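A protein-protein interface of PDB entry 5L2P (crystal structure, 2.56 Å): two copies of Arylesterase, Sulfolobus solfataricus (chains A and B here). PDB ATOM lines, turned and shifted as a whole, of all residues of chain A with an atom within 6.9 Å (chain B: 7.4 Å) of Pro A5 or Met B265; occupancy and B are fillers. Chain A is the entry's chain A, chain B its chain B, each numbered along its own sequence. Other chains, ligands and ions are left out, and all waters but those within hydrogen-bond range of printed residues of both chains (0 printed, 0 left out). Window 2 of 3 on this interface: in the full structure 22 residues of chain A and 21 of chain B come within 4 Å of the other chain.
Of chain B, only Met B265 comes within 4 Å of Pro A5. Printed residues of chain A within 4 Å of Tyr B262: Pro A2 (3.0 Å) and Leu A3 (3.8 Å). Of the printed residues of chain B, Pro A2 touches Tyr B262 (3.0 Å). The nearest printed residue of chain A that does not touch Thr B271 is Asp A4 (5.1 Å).
Hydrophobic or aromatic side chains of chain A within 4 Å of the printed part of chain B: Pro A2 and Pro A5. Of the 17 printed residues of chain B, 6 touch a printed residue of chain A. Printed residues of chain B that touch a printed residue of chain A: Glu B258, Tyr B262, Met B265, Thr B271, Leu B272 and Ser B273. Hydrophobic or aromatic side chains of chain B that line the printed part of chain A: Tyr B262 and Leu B272. Along chain B the printed residues that touch a printed residue of chain A span positions 258 to 273. Among the printed residues, no Asp or Glu carboxylate lies within 4 Å of a Lys or Arg side-chain nitrogen of the other chain.
The side-chain carboxylate of Glu B258 lies within hydrogen-bond range of the side-chain amide nitrogen of Asn A277 (3.1 Å). N of Asn A277 lies within hydrogen-bond range of O of Ser B273 (2.7 Å). The backbone carbonyl oxygen of Thr B271 is in hydrogen-bond range of the guanidinium group of Arg A288, at 3.2 Å.
NH2 of Arg A288 is in salt-bridge range of OD2 of Asp A4 (3.3 Å). O of Pro A5 sits close to OD1 of Asn A9. NH2 of Arg A288 lies within salt-bridge range of OE2 of Glu A6, at 2.9 Å. The backbone carbonyl oxygen of Asn A277 sits at hydrogen-bond distance from the side-chain amide nitrogen of Asn A279.
CZ of Tyr B262 touches CB of Pro A2, 3.0 Å away. Leu A3 touches Tyr B262 (O to CE1, 3.8 Å). CG of Pro A5 touches O of Met B265, 3.5 Å away. Leu B272 touches Thr A289 (CD1 to CG2, 3.8 Å).
No position is printed for both chains.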
ATOM      1  N   PRO A   2       7.526  -3.066  32.039  1.00  0.00           N
ATOM      2  CA  PRO A   2       7.520  -4.506  31.813  1.00  0.00           C
ATOM      3  C   PRO A   2       7.722  -4.874  30.336  1.00  0.00           C
ATOM      4  O   PRO A   2       6.783  -5.235  29.645  1.00  0.00           O
ATOM      5  CB  PRO A   2       6.146  -4.923  32.324  1.00  0.00           C
ATOM      6  CG  PRO A   2       5.292  -3.778  32.005  1.00  0.00           C
ATOM      7  CD  PRO A   2       6.151  -2.553  32.198  1.00  0.00           C
ATOM      8  N   LEU A   3       8.969  -4.788  29.879  1.00  0.00           N
ATOM      9  CA  LEU A   3       9.334  -5.221  28.547  1.00  0.00           C
ATOM     10  C   LEU A   3       9.904  -6.633  28.577  1.00  0.00           C
ATOM     11  O   LEU A   3      10.223  -7.179  29.623  1.00  0.00           O
ATOM     12  CB  LEU A   3      10.391  -4.281  27.947  1.00  0.00           C
ATOM     13  CG  LEU A   3      10.036  -2.808  27.793  1.00  0.00           C
ATOM     14  CD1 LEU A   3      11.284  -2.024  27.399  1.00  0.00           C
ATOM     15  CD2 LEU A   3       8.910  -2.646  26.760  1.00  0.00           C
ATOM     16  N   ASP A   4      10.016  -7.210  27.401  1.00  0.00           N
ATOM     17  CA  ASP A   4      10.855  -8.376  27.197  1.00  0.00           C
ATOM     18  C   ASP A   4      12.326  -8.050  27.625  1.00  0.00           C
ATOM     19  O   ASP A   4      12.881  -7.054  27.221  1.00  0.00           O
ATOM     20  CB  ASP A   4      10.781  -8.723  25.717  1.00  0.00           C
ATOM     21  CG  ASP A   4      11.384 -10.050  25.387  1.00  0.00           C
ATOM     22  OD1 ASP A   4      12.046 -10.705  26.235  1.00  0.00           O
ATOM     23  OD2 ASP A   4      11.177 -10.432  24.218  1.00  0.00           O
ATOM     24  N   PRO A   5      12.923  -8.883  28.471  1.00  0.00           N
ATOM     25  CA  PRO A   5      14.315  -8.640  28.917  1.00  0.00           C
ATOM     26  C   PRO A   5      15.347  -8.405  27.802  1.00  0.00           C
ATOM     27  O   PRO A   5      16.212  -7.575  27.957  1.00  0.00           O
ATOM     28  CB  PRO A   5      14.669  -9.916  29.704  1.00  0.00           C
ATOM     29  CG  PRO A   5      13.345 -10.364  30.251  1.00  0.00           C
ATOM     30  CD  PRO A   5      12.331 -10.048  29.166  1.00  0.00           C
ATOM     31  N   GLU A   6      15.249  -9.141  26.699  1.00  0.00           N
ATOM     32  CA  GLU A   6      16.137  -8.924  25.544  1.00  0.00           C
ATOM     33  C   GLU A   6      15.940  -7.537  24.954  1.00  0.00           C
ATOM     34  O   GLU A   6      16.891  -6.906  24.514  1.00  0.00           O
ATOM     35  CB  GLU A   6      15.995 -10.025  24.450  1.00  0.00           C
ATOM     36  CG  GLU A   6      14.592 -10.215  23.866  1.00  0.00           C
ATOM     37  CD  GLU A   6      14.440 -11.394  22.885  1.00  0.00           C
ATOM     38  OE1 GLU A   6      15.467 -11.807  22.260  1.00  0.00           O
ATOM     39  OE2 GLU A   6      13.283 -11.902  22.744  1.00  0.00           O
ATOM     40  N   VAL A   7      14.703  -7.058  24.941  1.00  0.00           N
ATOM     41  CA  VAL A   7      14.406  -5.719  24.425  1.00  0.00           C
ATOM     42  C   VAL A   7      14.930  -4.648  25.376  1.00  0.00           C
ATOM     43  O   VAL A   7      15.468  -3.640  24.954  1.00  0.00           O
ATOM     44  CB  VAL A   7      12.902  -5.531  24.186  1.00  0.00           C
ATOM     45  CG1 VAL A   7      12.587  -4.080  23.762  1.00  0.00           C
ATOM     46  CG2 VAL A   7      12.423  -6.521  23.128  1.00  0.00           C
ATOM     47  N   ARG A   8      14.746  -4.873  26.668  1.00  0.00           N
ATOM     48  CA  ARG A   8      15.236  -3.949  27.686  1.00  0.00           C
ATOM     49  C   ARG A   8      16.788  -3.808  27.604  1.00  0.00           C
ATOM     50  O   ARG A   8      17.319  -2.717  27.683  1.00  0.00           O
ATOM     51  CB  ARG A   8      14.853  -4.482  29.051  1.00  0.00           C
ATOM     52  CG  ARG A   8      15.078  -3.544  30.219  1.00  0.00           C
ATOM     53  CD  ARG A   8      14.886  -4.375  31.477  1.00  0.00           C
ATOM     54  NE  ARG A   8      14.861  -3.648  32.749  1.00  0.00           N
ATOM     55  CZ  ARG A   8      13.760  -3.232  33.385  1.00  0.00           C
ATOM     56  NH1 ARG A   8      12.543  -3.386  32.855  1.00  0.00           N
ATOM     57  NH2 ARG A   8      13.876  -2.616  34.554  1.00  0.00           N
ATOM     58  N   ASN A   9      17.480  -4.931  27.460  1.00  0.00           N
ATOM     59  CA  ASN A   9      18.907  -4.951  27.310  1.00  0.00           C
ATOM     60  C   ASN A   9      19.362  -4.197  26.033  1.00  0.00           C
ATOM     61  O   ASN A   9      20.353  -3.443  26.053  1.00  0.00           O
ATOM     62  CB  ASN A   9      19.418  -6.416  27.307  1.00  0.00           C
ATOM     63  CG  ASN A   9      19.288  -7.092  28.667  1.00  0.00           C
ATOM     64  OD1 ASN A   9      18.807  -6.479  29.636  1.00  0.00           O
ATOM     65  ND2 ASN A   9      19.732  -8.356  28.753  1.00  0.00           N
ATOM     66  N   PHE A  10      18.617  -4.383  24.948  1.00  0.00           N
ATOM     67  CA  PHE A  10      18.878  -3.664  23.715  1.00  0.00           C
ATOM     68  C   PHE A  10      18.809  -2.141  23.914  1.00  0.00           C
ATOM     69  O   PHE A  10      19.644  -1.392  23.384  1.00  0.00           O
ATOM     70  CB  PHE A  10      17.915  -4.134  22.593  1.00  0.00           C
ATOM     71  CG  PHE A  10      17.929  -3.257  21.372  1.00  0.00           C
ATOM     72  CD1 PHE A  10      18.946  -3.363  20.436  1.00  0.00           C
ATOM     73  CD2 PHE A  10      16.943  -2.292  21.183  1.00  0.00           C
ATOM     74  CE1 PHE A  10      18.974  -2.542  19.311  1.00  0.00           C
ATOM     75  CE2 PHE A  10      16.971  -1.446  20.082  1.00  0.00           C
ATOM     76  CZ  PHE A  10      17.986  -1.570  19.141  1.00  0.00           C
ATOM     77  N   GLN A  12      19.220  -0.370  26.671  1.00  0.00           N
ATOM     78  CA  GLN A  12      20.393   0.057  27.456  1.00  0.00           C
ATOM     79  C   GLN A  12      21.622   0.262  26.567  1.00  0.00           C
ATOM     80  O   GLN A  12      22.307   1.283  26.673  1.00  0.00           O
ATOM     81  CB  GLN A  12      20.714  -0.943  28.567  1.00  0.00           C
ATOM     82  CG  GLN A  12      19.651  -0.931  29.658  1.00  0.00           C
ATOM     83  CD  GLN A  12      19.651  -2.163  30.564  1.00  0.00           C
ATOM     84  OE1 GLN A  12      20.494  -3.057  30.446  1.00  0.00           O
ATOM     85  NE2 GLN A  12      18.672  -2.218  31.471  1.00  0.00           N
ATOM     86  N   ASN A 277       2.425  -7.574  22.617  1.00  0.00           N
ATOM     87  CA  ASN A 277       2.777  -7.067  23.923  1.00  0.00           C
ATOM     88  C   ASN A 277       4.286  -7.203  24.259  1.00  0.00           C
ATOM     89  O   ASN A 277       4.985  -8.031  23.717  1.00  0.00           O
ATOM     90  CB  ASN A 277       1.913  -7.734  24.995  1.00  0.00           C
ATOM     91  CG  ASN A 277       0.380  -7.442  24.834  1.00  0.00           C
ATOM     92  OD1 ASN A 277      -0.047  -6.344  24.474  1.00  0.00           O
ATOM     93  ND2 ASN A 277      -0.433  -8.452  25.101  1.00  0.00           N
ATOM     94  N   GLY A 278       4.758  -6.361  25.179  1.00  0.00           N
ATOM     95  CA  GLY A 278       6.108  -6.412  25.701  1.00  0.00           C
ATOM     96  C   GLY A 278       7.181  -6.029  24.704  1.00  0.00           C
ATOM     97  O   GLY A 278       8.363  -6.317  24.905  1.00  0.00           O
ATOM     98  N   ASN A 279       6.761  -5.322  23.659  1.00  0.00           N
ATOM     99  CA  ASN A 279       7.615  -4.932  22.573  1.00  0.00           C
ATOM    100  C   ASN A 279       7.494  -3.497  22.226  1.00  0.00           C
ATOM    101  O   ASN A 279       6.465  -2.885  22.460  1.00  0.00           O
ATOM    102  CB  ASN A 279       7.366  -5.772  21.340  1.00  0.00           C
ATOM    103  CG  ASN A 279       8.079  -7.122  21.404  1.00  0.00           C
ATOM    104  OD1 ASN A 279       9.196  -7.304  20.873  1.00  0.00           O
ATOM    105  ND2 ASN A 279       7.486  -8.031  22.129  1.00  0.00           N
ATOM    106  N   GLY A 285      15.220  -5.079  19.175  1.00  0.00           N
ATOM    107  CA  GLY A 285      15.794  -5.762  20.326  1.00  0.00           C
ATOM    108  C   GLY A 285      15.247  -7.174  20.543  1.00  0.00           C
ATOM    109  O   GLY A 285      15.615  -7.820  21.535  1.00  0.00           O
ATOM    110  N   ARG A 288      13.588 -12.644  17.547  1.00  0.00           N
ATOM    111  CA  ARG A 288      12.620 -13.755  17.647  1.00  0.00           C
ATOM    112  C   ARG A 288      11.179 -13.269  17.382  1.00  0.00           C
ATOM    113  O   ARG A 288      10.469 -13.843  16.571  1.00  0.00           O
ATOM    114  CB  ARG A 288      12.683 -14.442  19.035  1.00  0.00           C
ATOM    115  CG  ARG A 288      11.652 -15.572  19.219  1.00  0.00           C
ATOM    116  CD  ARG A 288      11.630 -16.197  20.632  1.00  0.00           C
ATOM    117  NE  ARG A 288      11.678 -15.167  21.673  1.00  0.00           N
ATOM    118  CZ  ARG A 288      10.637 -14.439  22.113  1.00  0.00           C
ATOM    119  NH1 ARG A 288       9.379 -14.615  21.636  1.00  0.00           N
ATOM    120  NH2 ARG A 288      10.849 -13.523  23.046  1.00  0.00           N
ATOM    121  N   THR A 289      10.767 -12.206  18.066  1.00  0.00           N
ATOM    122  CA  THR A 289       9.434 -11.618  17.837  1.00  0.00           C
ATOM    123  C   THR A 289       9.247 -11.089  16.419  1.00  0.00           C
ATOM    124  O   THR A 289       8.189 -11.260  15.796  1.00  0.00           O
ATOM    125  CB  THR A 289       9.161 -10.475  18.809  1.00  0.00           C
ATOM    126  OG1 THR A 289       9.345 -10.941  20.132  1.00  0.00           O
ATOM    127  CG2 THR A 289       7.765 -10.012  18.700  1.00  0.00           C
ATOM    128  N   LEU B 237       7.215 -19.023  38.143  1.00  0.00           N
ATOM    129  CA  LEU B 237       6.808 -19.285  36.796  1.00  0.00           C
ATOM    130  C   LEU B 237       7.947 -19.452  35.791  1.00  0.00           C
ATOM    131  O   LEU B 237       7.718 -19.313  34.585  1.00  0.00           O
ATOM    132  CB  LEU B 237       5.851 -18.172  36.356  1.00  0.00           C
ATOM    133  CG  LEU B 237       4.487 -18.243  37.070  1.00  0.00           C
ATOM    134  CD1 LEU B 237       3.682 -17.032  36.676  1.00  0.00           C
ATOM    135  CD2 LEU B 237       3.692 -19.505  36.780  1.00  0.00           C
ATOM    136  N   GLU B 258      -2.641 -11.172  29.875  1.00  0.00           N
ATOM    137  CA  GLU B 258      -1.470 -10.369  29.587  1.00  0.00           C
ATOM    138  C   GLU B 258      -0.502 -10.340  30.766  1.00  0.00           C
ATOM    139  O   GLU B 258       0.708 -10.331  30.581  1.00  0.00           O
ATOM    140  CB  GLU B 258      -1.872  -8.987  29.117  1.00  0.00           C
ATOM    141  CG  GLU B 258      -2.515  -9.092  27.718  1.00  0.00           C
ATOM    142  CD  GLU B 258      -3.007  -7.771  27.151  1.00  0.00           C
ATOM    143  OE1 GLU B 258      -3.169  -6.741  27.898  1.00  0.00           O
ATOM    144  OE2 GLU B 258      -3.333  -7.789  25.943  1.00  0.00           O
ATOM    145  N   ALA B 259      -1.032 -10.355  31.969  1.00  0.00           N
ATOM    146  CA  ALA B 259      -0.221 -10.431  33.152  1.00  0.00           C
ATOM    147  C   ALA B 259       0.535 -11.759  33.269  1.00  0.00           C
ATOM    148  O   ALA B 259       1.682 -11.789  33.715  1.00  0.00           O
ATOM    149  CB  ALA B 259      -1.127 -10.257  34.351  1.00  0.00           C
ATOM    150  N   TYR B 260      -0.120 -12.859  32.919  1.00  0.00           N
ATOM    151  CA  TYR B 260       0.497 -14.171  32.926  1.00  0.00           C
ATOM    152  C   TYR B 260       1.697 -14.211  31.934  1.00  0.00           C
ATOM    153  O   TYR B 260       2.767 -14.686  32.244  1.00  0.00           O
ATOM    154  CB  TYR B 260      -0.546 -15.251  32.548  1.00  0.00           C
ATOM    155  CG  TYR B 260       0.020 -16.661  32.635  1.00  0.00           C
ATOM    156  CD1 TYR B 260       0.328 -17.255  33.860  1.00  0.00           C
ATOM    157  CD2 TYR B 260       0.271 -17.383  31.507  1.00  0.00           C
ATOM    158  CE1 TYR B 260       0.885 -18.538  33.932  1.00  0.00           C
ATOM    159  CE2 TYR B 260       0.819 -18.664  31.570  1.00  0.00           C
ATOM    160  CZ  TYR B 260       1.141 -19.230  32.774  1.00  0.00           C
ATOM    161  OH  TYR B 260       1.658 -20.536  32.791  1.00  0.00           O
ATOM    162  N   ALA B 261       1.466 -13.654  30.748  1.00  0.00           N
ATOM    163  CA  ALA B 261       2.451 -13.535  29.733  1.00  0.00           C
ATOM    164  C   ALA B 261       3.659 -12.693  30.185  1.00  0.00           C
ATOM    165  O   ALA B 261       4.794 -13.077  29.937  1.00  0.00           O
ATOM    166  CB  ALA B 261       1.832 -12.979  28.477  1.00  0.00           C
ATOM    167  N   TYR B 262       3.412 -11.584  30.861  1.00  0.00           N
ATOM    168  CA  TYR B 262       4.525 -10.775  31.363  1.00  0.00           C
ATOM    169  C   TYR B 262       5.331 -11.518  32.436  1.00  0.00           C
ATOM    170  O   TYR B 262       6.551 -11.451  32.459  1.00  0.00           O
ATOM    171  CB  TYR B 262       4.085  -9.393  31.893  1.00  0.00           C
ATOM    172  CG  TYR B 262       5.266  -8.634  32.471  1.00  0.00           C
ATOM    173  CD1 TYR B 262       6.413  -8.392  31.690  1.00  0.00           C
ATOM    174  CD2 TYR B 262       5.285  -8.213  33.801  1.00  0.00           C
ATOM    175  CE1 TYR B 262       7.516  -7.732  32.197  1.00  0.00           C
ATOM    176  CE2 TYR B 262       6.394  -7.545  34.318  1.00  0.00           C
ATOM    177  CZ  TYR B 262       7.507  -7.308  33.513  1.00  0.00           C
ATOM    178  OH  TYR B 262       8.622  -6.632  34.013  1.00  0.00           O
ATOM    179  N   ARG B 263       4.633 -12.212  33.321  1.00  0.00           N
ATOM    180  CA  ARG B 263       5.278 -12.950  34.396  1.00  0.00           C
ATOM    181  C   ARG B 263       6.180 -14.016  33.832  1.00  0.00           C
ATOM    182  O   ARG B 263       7.246 -14.276  34.378  1.00  0.00           O
ATOM    183  CB  ARG B 263       4.234 -13.595  35.330  1.00  0.00           C
ATOM    184  CG  ARG B 263       3.655 -12.678  36.402  1.00  0.00           C
ATOM    185  CD  ARG B 263       4.304 -12.901  37.769  1.00  0.00           C
ATOM    186  NE  ARG B 263       3.512 -13.785  38.645  1.00  0.00           N
ATOM    187  CZ  ARG B 263       4.009 -14.748  39.434  1.00  0.00           C
ATOM    188  NH1 ARG B 263       5.318 -14.998  39.501  1.00  0.00           N
ATOM    189  NH2 ARG B 263       3.188 -15.471  40.180  1.00  0.00           N
ATOM    190  N   LEU B 264       5.746 -14.647  32.741  1.00  0.00           N
ATOM    191  CA  LEU B 264       6.577 -15.621  32.041  1.00  0.00           C
ATOM    192  C   LEU B 264       7.854 -14.947  31.472  1.00  0.00           C
ATOM    193  O   LEU B 264       8.961 -15.478  31.649  1.00  0.00           O
ATOM    194  CB  LEU B 264       5.819 -16.313  30.931  1.00  0.00           C
ATOM    195  CG  LEU B 264       4.724 -17.318  31.384  1.00  0.00           C
ATOM    196  CD1 LEU B 264       3.931 -17.844  30.199  1.00  0.00           C
ATOM    197  CD2 LEU B 264       5.249 -18.515  32.148  1.00  0.00           C
ATOM    198  N   MET B 265       7.709 -13.788  30.823  1.00  0.00           N
ATOM    199  CA  MET B 265       8.850 -13.046  30.320  1.00  0.00           C
ATOM    200  C   MET B 265       9.854 -12.689  31.400  1.00  0.00           C
ATOM    201  O   MET B 265      11.075 -12.841  31.204  1.00  0.00           O
ATOM    202  CB  MET B 265       8.422 -11.763  29.627  1.00  0.00           C
ATOM    203  CG  MET B 265       7.826 -11.960  28.259  1.00  0.00           C
ATOM    204  SD  MET B 265       7.354 -10.369  27.561  1.00  0.00           S
ATOM    205  CE  MET B 265       6.557 -10.948  26.043  1.00  0.00           C
ATOM    206  N   GLU B 266       9.350 -12.199  32.527  1.00  0.00           N
ATOM    207  CA  GLU B 266      10.227 -11.898  33.658  1.00  0.00           C
ATOM    208  C   GLU B 266      10.965 -13.105  34.198  1.00  0.00           C
ATOM    209  O   GLU B 266      11.999 -12.952  34.761  1.00  0.00           O
ATOM    210  CB  GLU B 266       9.441 -11.381  34.833  1.00  0.00           C
ATOM    211  CG  GLU B 266       8.977  -9.986  34.694  1.00  0.00           C
ATOM    212  CD  GLU B 266       8.256  -9.564  35.955  1.00  0.00           C
ATOM    213  OE1 GLU B 266       8.972  -9.076  36.872  1.00  0.00           O
ATOM    214  OE2 GLU B 266       7.005  -9.781  36.045  1.00  0.00           O
ATOM    215  N   SER B 267      10.349 -14.280  34.098  1.00  0.00           N
ATOM    216  CA  SER B 267      10.901 -15.501  34.638  1.00  0.00           C
ATOM    217  C   SER B 267      11.859 -16.164  33.660  1.00  0.00           C
ATOM    218  O   SER B 267      12.264 -17.304  33.891  1.00  0.00           O
ATOM    219  CB  SER B 267       9.765 -16.484  34.967  1.00  0.00           C
ATOM    220  OG  SER B 267       8.866 -15.926  35.895  1.00  0.00           O
ATOM    221  N   GLY B 268      12.183 -15.495  32.550  1.00  0.00           N
ATOM    222  CA  GLY B 268      13.060 -16.067  31.531  1.00  0.00           C
ATOM    223  C   GLY B 268      12.457 -17.000  30.511  1.00  0.00           C
ATOM    224  O   GLY B 268      13.152 -17.632  29.795  1.00  0.00           O
ATOM    225  N   VAL B 269      11.132 -17.102  30.443  1.00  0.00           N
ATOM    226  CA  VAL B 269      10.486 -18.000  29.468  1.00  0.00           C
ATOM    227  C   VAL B 269      10.289 -17.235  28.164  1.00  0.00           C
ATOM    228  O   VAL B 269       9.750 -16.148  28.189  1.00  0.00           O
ATOM    229  CB  VAL B 269       9.155 -18.535  29.976  1.00  0.00           C
ATOM    230  CG1 VAL B 269       8.508 -19.412  28.911  1.00  0.00           C
ATOM    231  CG2 VAL B 269       9.362 -19.316  31.255  1.00  0.00           C
ATOM    232  N   PRO B 270      10.762 -17.772  27.021  1.00  0.00           N
ATOM    233  CA  PRO B 270      10.522 -17.065  25.758  1.00  0.00           C
ATOM    234  C   PRO B 270       9.034 -17.098  25.440  1.00  0.00           C
ATOM    235  O   PRO B 270       8.427 -18.192  25.379  1.00  0.00           O
ATOM    236  CB  PRO B 270      11.309 -17.873  24.705  1.00  0.00           C
ATOM    237  CG  PRO B 270      12.022 -18.971  25.425  1.00  0.00           C
ATOM    238  CD  PRO B 270      11.598 -18.982  26.863  1.00  0.00           C
ATOM    239  N   THR B 271       8.445 -15.919  25.255  1.00  0.00           N
ATOM    240  CA  THR B 271       7.018 -15.830  25.014  1.00  0.00           C
ATOM    241  C   THR B 271       6.665 -14.782  23.982  1.00  0.00           C
ATOM    242  O   THR B 271       7.262 -13.720  23.901  1.00  0.00           O
ATOM    243  CB  THR B 271       6.197 -15.543  26.318  1.00  0.00           C
ATOM    244  OG1 THR B 271       6.482 -14.235  26.794  1.00  0.00           O
ATOM    245  CG2 THR B 271       6.496 -16.525  27.460  1.00  0.00           C
ATOM    246  N   LEU B 272       5.685 -15.130  23.176  1.00  0.00           N
ATOM    247  CA  LEU B 272       4.979 -14.182  22.332  1.00  0.00           C
ATOM    248  C   LEU B 272       3.566 -13.982  22.938  1.00  0.00           C
ATOM    249  O   LEU B 272       2.896 -14.909  23.369  1.00  0.00           O
ATOM    250  CB  LEU B 272       4.867 -14.710  20.921  1.00  0.00           C
ATOM    251  CG  LEU B 272       4.215 -13.728  19.957  1.00  0.00           C
ATOM    252  CD1 LEU B 272       5.126 -12.545  19.645  1.00  0.00           C
ATOM    253  CD2 LEU B 272       3.820 -14.437  18.659  1.00  0.00           C
ATOM    254  N   SER B 273       3.155 -12.735  23.015  1.00  0.00           N
ATOM    255  CA  SER B 273       1.905 -12.369  23.616  1.00  0.00           C
ATOM    256  C   SER B 273       1.290 -11.311  22.734  1.00  0.00           C
ATOM    257  O   SER B 273       1.868 -10.261  22.518  1.00  0.00           O
ATOM    258  CB  SER B 273       2.164 -11.831  24.998  1.00  0.00           C
ATOM    259  OG  SER B 273       1.013 -11.317  25.561  1.00  0.00           O
